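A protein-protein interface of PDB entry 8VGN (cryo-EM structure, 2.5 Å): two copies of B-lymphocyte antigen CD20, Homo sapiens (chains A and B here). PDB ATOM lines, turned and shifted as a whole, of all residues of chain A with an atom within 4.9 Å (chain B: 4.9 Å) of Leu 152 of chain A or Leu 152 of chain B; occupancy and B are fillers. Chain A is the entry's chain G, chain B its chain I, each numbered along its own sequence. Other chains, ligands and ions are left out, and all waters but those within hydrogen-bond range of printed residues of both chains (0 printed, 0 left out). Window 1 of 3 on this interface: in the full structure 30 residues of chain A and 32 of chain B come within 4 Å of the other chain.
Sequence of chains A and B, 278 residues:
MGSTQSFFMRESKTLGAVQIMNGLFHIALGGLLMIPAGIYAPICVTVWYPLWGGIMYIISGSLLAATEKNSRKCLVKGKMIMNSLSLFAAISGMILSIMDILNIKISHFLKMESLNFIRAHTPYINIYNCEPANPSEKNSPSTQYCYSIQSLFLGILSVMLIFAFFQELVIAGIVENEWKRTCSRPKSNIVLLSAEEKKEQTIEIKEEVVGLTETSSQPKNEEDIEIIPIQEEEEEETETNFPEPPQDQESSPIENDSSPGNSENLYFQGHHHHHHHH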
ATOM      1  N   LEU A  32      32.519  29.507  23.327  1.00  0.00           N
ATOM      2  CA  LEU A  32      31.259  28.911  22.907  1.00  0.00           C
ATOM      3  C   LEU A  32      31.467  27.537  22.287  1.00  0.00           C
ATOM      4  O   LEU A  32      30.701  26.606  22.548  1.00  0.00           O
ATOM      5  CB  LEU A  32      30.584  29.854  21.918  1.00  0.00           C
ATOM      6  CG  LEU A  32      29.189  29.562  21.423  1.00  0.00           C
ATOM      7  CD1 LEU A  32      28.248  29.898  22.527  1.00  0.00           C
ATOM      8  CD2 LEU A  32      28.923  30.431  20.226  1.00  0.00           C
ATOM      9  N   ILE A  35      31.962  24.655  24.746  1.00  0.00           N
ATOM     10  CA  ILE A  35      30.844  24.091  25.509  1.00  0.00           C
ATOM     11  C   ILE A  35      30.768  22.593  25.250  1.00  0.00           C
ATOM     12  O   ILE A  35      30.756  22.168  24.079  1.00  0.00           O
ATOM     13  CB  ILE A  35      29.528  24.782  25.131  1.00  0.00           C
ATOM     14  CG1 ILE A  35      29.520  26.215  25.659  1.00  0.00           C
ATOM     15  CG2 ILE A  35      28.348  24.005  25.663  1.00  0.00           C
ATOM     16  CD1 ILE A  35      28.369  27.042  25.163  1.00  0.00           C
ATOM     17  N   SER A 148      21.637  18.329  15.095  1.00  0.00           N
ATOM     18  CA  SER A 148      21.572  19.727  15.514  1.00  0.00           C
ATOM     19  C   SER A 148      22.911  20.234  16.038  1.00  0.00           C
ATOM     20  O   SER A 148      23.346  21.331  15.680  1.00  0.00           O
ATOM     21  CB  SER A 148      20.479  19.915  16.559  1.00  0.00           C
ATOM     22  OG  SER A 148      19.234  19.475  16.059  1.00  0.00           O
ATOM     23  N   ILE A 149      23.578  19.461  16.893  1.00  0.00           N
ATOM     24  CA  ILE A 149      24.872  19.899  17.408  1.00  0.00           C
ATOM     25  C   ILE A 149      25.906  19.952  16.296  1.00  0.00           C
ATOM     26  O   ILE A 149      26.708  20.888  16.221  1.00  0.00           O
ATOM     27  CB  ILE A 149      25.349  18.982  18.545  1.00  0.00           C
ATOM     28  CG1 ILE A 149      24.303  18.868  19.634  1.00  0.00           C
ATOM     29  CG2 ILE A 149      26.621  19.515  19.149  1.00  0.00           C
ATOM     30  CD1 ILE A 149      24.443  17.634  20.453  1.00  0.00           C
ATOM     31  N   GLN A 150      25.914  18.948  15.426  1.00  0.00           N
ATOM     32  CA  GLN A 150      26.831  18.951  14.295  1.00  0.00           C
ATOM     33  C   GLN A 150      26.622  20.162  13.395  1.00  0.00           C
ATOM     34  O   GLN A 150      27.588  20.733  12.882  1.00  0.00           O
ATOM     35  CB  GLN A 150      26.674  17.653  13.513  1.00  0.00           C
ATOM     36  CG  GLN A 150      27.702  17.452  12.440  1.00  0.00           C
ATOM     37  CD  GLN A 150      27.374  16.282  11.558  1.00  0.00           C
ATOM     38  OE1 GLN A 150      26.749  16.435  10.512  1.00  0.00           O
ATOM     39  NE2 GLN A 150      27.801  15.098  11.968  1.00  0.00           N
ATOM     40  N   SER A 151      25.371  20.564  13.184  1.00  0.00           N
ATOM     41  CA  SER A 151      25.100  21.758  12.389  1.00  0.00           C
ATOM     42  C   SER A 151      25.513  23.041  13.100  1.00  0.00           C
ATOM     43  O   SER A 151      26.010  23.972  12.459  1.00  0.00           O
ATOM     44  CB  SER A 151      23.623  21.813  12.022  1.00  0.00           C
ATOM     45  OG  SER A 151      23.233  20.639  11.341  1.00  0.00           O
ATOM     46  N   LEU A 152      25.307  23.121  14.414  1.00  0.00           N
ATOM     47  CA  LEU A 152      25.806  24.266  15.170  1.00  0.00           C
ATOM     48  C   LEU A 152      27.323  24.378  15.133  1.00  0.00           C
ATOM     49  O   LEU A 152      27.859  25.472  14.944  1.00  0.00           O
ATOM     50  CB  LEU A 152      25.328  24.190  16.616  1.00  0.00           C
ATOM     51  CG  LEU A 152      23.864  24.518  16.861  1.00  0.00           C
ATOM     52  CD1 LEU A 152      23.446  24.026  18.224  1.00  0.00           C
ATOM     53  CD2 LEU A 152      23.671  26.008  16.761  1.00  0.00           C
ATOM     54  N   PHE A 153      28.034  23.268  15.314  1.00  0.00           N
ATOM     55  CA  PHE A 153      29.488  23.310  15.213  1.00  0.00           C
ATOM     56  C   PHE A 153      29.948  23.732  13.828  1.00  0.00           C
ATOM     57  O   PHE A 153      30.855  24.556  13.688  1.00  0.00           O
ATOM     58  CB  PHE A 153      30.078  21.958  15.591  1.00  0.00           C
ATOM     59  CG  PHE A 153      30.449  21.864  17.026  1.00  0.00           C
ATOM     60  CD1 PHE A 153      29.486  21.945  18.007  1.00  0.00           C
ATOM     61  CD2 PHE A 153      31.768  21.727  17.400  1.00  0.00           C
ATOM     62  CE1 PHE A 153      29.832  21.874  19.331  1.00  0.00           C
ATOM     63  CE2 PHE A 153      32.116  21.654  18.722  1.00  0.00           C
ATOM     64  CZ  PHE A 153      31.149  21.730  19.687  1.00  0.00           C
ATOM     65  N   LEU A 154      29.341  23.170  12.790  1.00  0.00           N
ATOM     66  CA  LEU A 154      29.634  23.608  11.432  1.00  0.00           C
ATOM     67  C   LEU A 154      29.341  25.093  11.239  1.00  0.00           C
ATOM     68  O   LEU A 154      30.051  25.782  10.500  1.00  0.00           O
ATOM     69  CB  LEU A 154      28.837  22.759  10.447  1.00  0.00           C
ATOM     70  CG  LEU A 154      29.021  23.038   8.964  1.00  0.00           C
ATOM     71  CD1 LEU A 154      30.448  22.734   8.578  1.00  0.00           C
ATOM     72  CD2 LEU A 154      28.066  22.191   8.161  1.00  0.00           C
ATOM     73  N   GLY A 155      28.295  25.599  11.891  1.00  0.00           N
ATOM     74  CA  GLY A 155      28.026  27.030  11.864  1.00  0.00           C
ATOM     75  C   GLY A 155      29.046  27.885  12.596  1.00  0.00           C
ATOM     76  O   GLY A 155      29.524  28.886  12.063  1.00  0.00           O
ATOM     77  N   ILE A 156      29.386  27.510  13.831  1.00  0.00           N
ATOM     78  CA  ILE A 156      30.367  28.267  14.608  1.00  0.00           C
ATOM     79  C   ILE A 156      31.730  28.267  13.933  1.00  0.00           C
ATOM     80  O   ILE A 156      32.421  29.290  13.904  1.00  0.00           O
ATOM     81  CB  ILE A 156      30.463  27.718  16.043  1.00  0.00           C
ATOM     82  CG1 ILE A 156      29.135  27.859  16.772  1.00  0.00           C
ATOM     83  CG2 ILE A 156      31.537  28.445  16.810  1.00  0.00           C
ATOM     84  CD1 ILE A 156      29.028  26.989  17.990  1.00  0.00           C
ATOM     85  N   LEU A 157      32.144  27.128  13.388  1.00  0.00           N
ATOM     86  CA  LEU A 157      33.423  27.060  12.694  1.00  0.00           C
ATOM     87  C   LEU A 157      33.449  27.942  11.454  1.00  0.00           C
ATOM     88  O   LEU A 157      34.459  28.593  11.173  1.00  0.00           O
ATOM     89  CB  LEU A 157      33.740  25.614  12.332  1.00  0.00           C
ATOM     90  CG  LEU A 157      34.068  24.735  13.532  1.00  0.00           C
ATOM     91  CD1 LEU A 157      33.998  23.279  13.152  1.00  0.00           C
ATOM     92  CD2 LEU A 157      35.433  25.086  14.070  1.00  0.00           C
ATOM     93  N   LEU B  32      23.430  31.946  13.292  1.00  0.00           N
ATOM     94  CA  LEU B  32      23.876  30.765  14.017  1.00  0.00           C
ATOM     95  C   LEU B  32      22.800  30.246  14.960  1.00  0.00           C
ATOM     96  O   LEU B  32      22.590  29.035  15.071  1.00  0.00           O
ATOM     97  CB  LEU B  32      25.143  31.117  14.785  1.00  0.00           C
ATOM     98  CG  LEU B  32      25.912  30.044  15.515  1.00  0.00           C
ATOM     99  CD1 LEU B  32      26.634  29.241  14.491  1.00  0.00           C
ATOM    100  CD2 LEU B  32      26.887  30.715  16.443  1.00  0.00           C
ATOM    101  N   ILE B  35      20.032  28.164  13.341  1.00  0.00           N
ATOM    102  CA  ILE B  35      20.263  26.781  12.911  1.00  0.00           C
ATOM    103  C   ILE B  35      19.243  25.872  13.580  1.00  0.00           C
ATOM    104  O   ILE B  35      19.088  25.921  14.815  1.00  0.00           O
ATOM    105  CB  ILE B  35      21.694  26.343  13.249  1.00  0.00           C
ATOM    106  CG1 ILE B  35      22.693  27.081  12.361  1.00  0.00           C
ATOM    107  CG2 ILE B  35      21.841  24.848  13.098  1.00  0.00           C
ATOM    108  CD1 ILE B  35      24.128  26.856  12.744  1.00  0.00           C
ATOM    109  N   SER B 148      23.421  19.297  25.576  1.00  0.00           N
ATOM    110  CA  SER B 148      24.443  19.996  24.800  1.00  0.00           C
ATOM    111  C   SER B 148      23.863  21.152  23.994  1.00  0.00           C
ATOM    112  O   SER B 148      24.428  22.248  23.978  1.00  0.00           O
ATOM    113  CB  SER B 148      25.175  19.019  23.888  1.00  0.00           C
ATOM    114  OG  SER B 148      25.741  17.967  24.641  1.00  0.00           O
ATOM    115  N   ILE B 149      22.742  20.932  23.308  1.00  0.00           N
ATOM    116  CA  ILE B 149      22.142  22.016  22.536  1.00  0.00           C
ATOM    117  C   ILE B 149      21.637  23.117  23.453  1.00  0.00           C
ATOM    118  O   ILE B 149      21.807  24.305  23.169  1.00  0.00           O
ATOM    119  CB  ILE B 149      21.004  21.491  21.645  1.00  0.00           C
ATOM    120  CG1 ILE B 149      21.478  20.350  20.769  1.00  0.00           C
ATOM    121  CG2 ILE B 149      20.479  22.592  20.764  1.00  0.00           C
ATOM    122  CD1 ILE B 149      20.372  19.466  20.309  1.00  0.00           C
ATOM    123  N   GLN B 150      21.002  22.743  24.558  1.00  0.00           N
ATOM    124  CA  GLN B 150      20.539  23.732  25.522  1.00  0.00           C
ATOM    125  C   GLN B 150      21.684  24.571  26.072  1.00  0.00           C
ATOM    126  O   GLN B 150      21.531  25.776  26.285  1.00  0.00           O
ATOM    127  CB  GLN B 150      19.786  23.031  26.646  1.00  0.00           C
ATOM    128  CG  GLN B 150      19.093  23.961  27.596  1.00  0.00           C
ATOM    129  CD  GLN B 150      18.561  23.239  28.802  1.00  0.00           C
ATOM    130  OE1 GLN B 150      19.224  23.162  29.833  1.00  0.00           O
ATOM    131  NE2 GLN B 150      17.353  22.711  28.687  1.00  0.00           N
ATOM    132  N   SER B 151      22.837  23.955  26.317  1.00  0.00           N
ATOM    133  CA  SER B 151      24.000  24.707  26.780  1.00  0.00           C
ATOM    134  C   SER B 151      24.582  25.608  25.698  1.00  0.00           C
ATOM    135  O   SER B 151      25.019  26.725  25.990  1.00  0.00           O
ATOM    136  CB  SER B 151      25.065  23.751  27.299  1.00  0.00           C
ATOM    137  OG  SER B 151      24.544  22.928  28.321  1.00  0.00           O
ATOM    138  N   LEU B 152      24.611  25.145  24.449  1.00  0.00           N
ATOM    139  CA  LEU B 152      25.030  26.011  23.351  1.00  0.00           C
ATOM    140  C   LEU B 152      24.112  27.210  23.168  1.00  0.00           C
ATOM    141  O   LEU B 152      24.587  28.332  22.980  1.00  0.00           O
ATOM    142  CB  LEU B 152      25.108  25.215  22.053  1.00  0.00           C
ATOM    143  CG  LEU B 152      26.290  24.268  21.913  1.00  0.00           C
ATOM    144  CD1 LEU B 152      26.032  23.282  20.803  1.00  0.00           C
ATOM    145  CD2 LEU B 152      27.531  25.072  21.624  1.00  0.00           C
ATOM    146  N   PHE B 153      22.798  27.002  23.211  1.00  0.00           N
ATOM    147  CA  PHE B 153      21.878  28.129  23.116  1.00  0.00           C
ATOM    148  C   PHE B 153      22.060  29.107  24.264  1.00  0.00           C
ATOM    149  O   PHE B 153      22.087  30.324  24.059  1.00  0.00           O
ATOM    150  CB  PHE B 153      20.442  27.626  23.052  1.00  0.00           C
ATOM    151  CG  PHE B 153      19.945  27.450  21.664  1.00  0.00           C
ATOM    152  CD1 PHE B 153      20.519  26.522  20.825  1.00  0.00           C
ATOM    153  CD2 PHE B 153      18.922  28.237  21.181  1.00  0.00           C
ATOM    154  CE1 PHE B 153      20.072  26.370  19.540  1.00  0.00           C
ATOM    155  CE2 PHE B 153      18.471  28.087  19.897  1.00  0.00           C
ATOM    156  CZ  PHE B 153      19.047  27.155  19.075  1.00  0.00           C
ATOM    157  N   LEU B 154      22.178  28.596  25.483  1.00  0.00           N
ATOM    158  CA  LEU B 154      22.479  29.455  26.620  1.00  0.00           C
ATOM    159  C   LEU B 154      23.794  30.206  26.432  1.00  0.00           C
ATOM    160  O   LEU B 154      23.925  31.357  26.857  1.00  0.00           O
ATOM    161  CB  LEU B 154      22.504  28.615  27.893  1.00  0.00           C
ATOM    162  CG  LEU B 154      22.775  29.330  29.206  1.00  0.00           C
ATOM    163  CD1 LEU B 154      21.653  30.302  29.478  1.00  0.00           C
ATOM    164  CD2 LEU B 154      22.884  28.322  30.323  1.00  0.00           C
ATOM    165  N   GLY B 155      24.779  29.567  25.802  1.00  0.00           N
ATOM    166  CA  GLY B 155      26.016  30.257  25.466  1.00  0.00           C
ATOM    167  C   GLY B 155      25.877  31.336  24.407  1.00  0.00           C
ATOM    168  O   GLY B 155      26.366  32.453  24.581  1.00  0.00           O
ATOM    169  N   ILE B 156      25.219  31.018  23.291  1.00  0.00           N
ATOM    170  CA  ILE B 156      25.030  31.994  22.218  1.00  0.00           C
ATOM    171  C   ILE B 156      24.213  33.187  22.692  1.00  0.00           C
ATOM    172  O   ILE B 156      24.513  34.335  22.351  1.00  0.00           O
ATOM    173  CB  ILE B 156      24.382  31.334  20.990  1.00  0.00           C
ATOM    174  CG1 ILE B 156      25.276  30.241  20.421  1.00  0.00           C
ATOM    175  CG2 ILE B 156      24.111  32.364  19.923  1.00  0.00           C
ATOM    176  CD1 ILE B 156      24.553  29.291  19.512  1.00  0.00           C
ATOM    177  N   LEU B 157      23.168  32.940  23.473  1.00  0.00           N
ATOM    178  CA  LEU B 157      22.357  34.034  23.994  1.00  0.00           C
ATOM    179  C   LEU B 157      23.148  34.935  24.932  1.00  0.00           C
ATOM    180  O   LEU B 157      22.995  36.158  24.894  1.00  0.00           O
ATOM    181  CB  LEU B 157      21.124  33.477  24.696  1.00  0.00           C
ATOM    182  CG  LEU B 157      20.109  32.849  23.748  1.00  0.00           C
ATOM    183  CD1 LEU B 157      19.126  32.005  24.517  1.00  0.00           C
ATOM    184  CD2 LEU B 157      19.397  33.927  22.968  1.00  0.00           C
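Leu 152 of chain B touches just these residues of chain A: Leu 32, Ile 35 and Leu 152. Of the printed residues of chain B, Ile 35 of chain A touches Ser 151, Leu 152 and Gly 155. Of the printed residues of chain A, Ser 151 of chain B touches Ile 35. Printed residues of chain A within 4 Å of Ile 35 of chain B: Ser 151, Leu 152 and Gly 155. Printed residues of chain A within 4 Å of Ser 148 of chain B: Ile 149 (3.8 Å). Of the printed residues of chain B, Gly 155 of chain A touches Leu 32 and Ile 35. Leu 154 of chain A touches none of the printed residues of chain B. Phe 153 of chain A touches none of the printed residues of chain B. The nearest residue of chain A that does not touch Leu 152 of chain B is Ile 149 of chain A (4.2 Å).
Leu 32 of chain A touches Gly 155 of chain B, and with the chains exchanged Gly 155 of chain A touches Leu 32 of chain B. Ile 35 of chain A touches Ser 151 of chain B, and with the chains exchanged Ser 151 of chain A touches Ile 35 of chain B. Ser 148 of chain A touches Ile 149 of chain B, and with the chains exchanged Ile 149 of chain A touches Ser 148 of chain B. Leu 152 of chain A touches its own counterpart, Leu 152 of chain B.
Among the printed residues, merely in contact across the chains: Leu 32 of chain A with Leu 152 of chain B (3.6 Å), Leu 32 of chain A with Gly 155 of chain B (3.4 Å), Leu 32 of chain A with Ile 156 of chain B (3.3 Å), Ile 35 of chain A with Ser 151 of chain B (3.5 Å), Ile 35 of chain A with Leu 152 of chain B (3.9 Å), Ile 35 of chain A with Gly 155 of chain B (3.996 Å), Ser 148 of chain A with Ile 149 of chain B (3.8 Å), Ile 149 of chain A with Ser 148 of chain B (3.8 Å), Ile 149 of chain A with Ile 149 of chain B (3.4 Å), Ser 151 of chain A with Ile 35 of chain B (3.5 Å), Leu 152 of chain A with Leu 32 of chain B (3.6 Å), Leu 152 of chain A with Ile 35 of chain B (3.9 Å), Leu 152 of chain A with Leu 152 of chain B (3.7 Å), Gly 155 of chain A with Leu 32 of chain B (3.4 Å), Gly 155 of chain A with Ile 35 of chain B (3.9999 Å) and Ile 156 of chain A with Leu 32 of chain B (3.3 Å).
Of the 12 printed residues of chain A, 8 touch a printed residue of chain B. Printed residues of chain A that touch a printed residue of chain B: Leu 32, Ile 35, Ser 148, Ile 149, Ser 151, Leu 152, Gly 155 and Ile 156. Hydrophobic or aromatic side chains of chain A that line the printed part of chain B: Leu 32, Ile 35, Ile 149, Leu 152 and Ile 156. Hydrophobic or aromatic side chains of chain B within 4 Å of the printed part of chain A: Leu 32, Ile 35, Ile 149, Leu 152 and Ile 156. Among the printed residues, no Asp or Glu carboxylate lies within 4 Å of a Lys or Arg side-chain nitrogen of the other chain.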
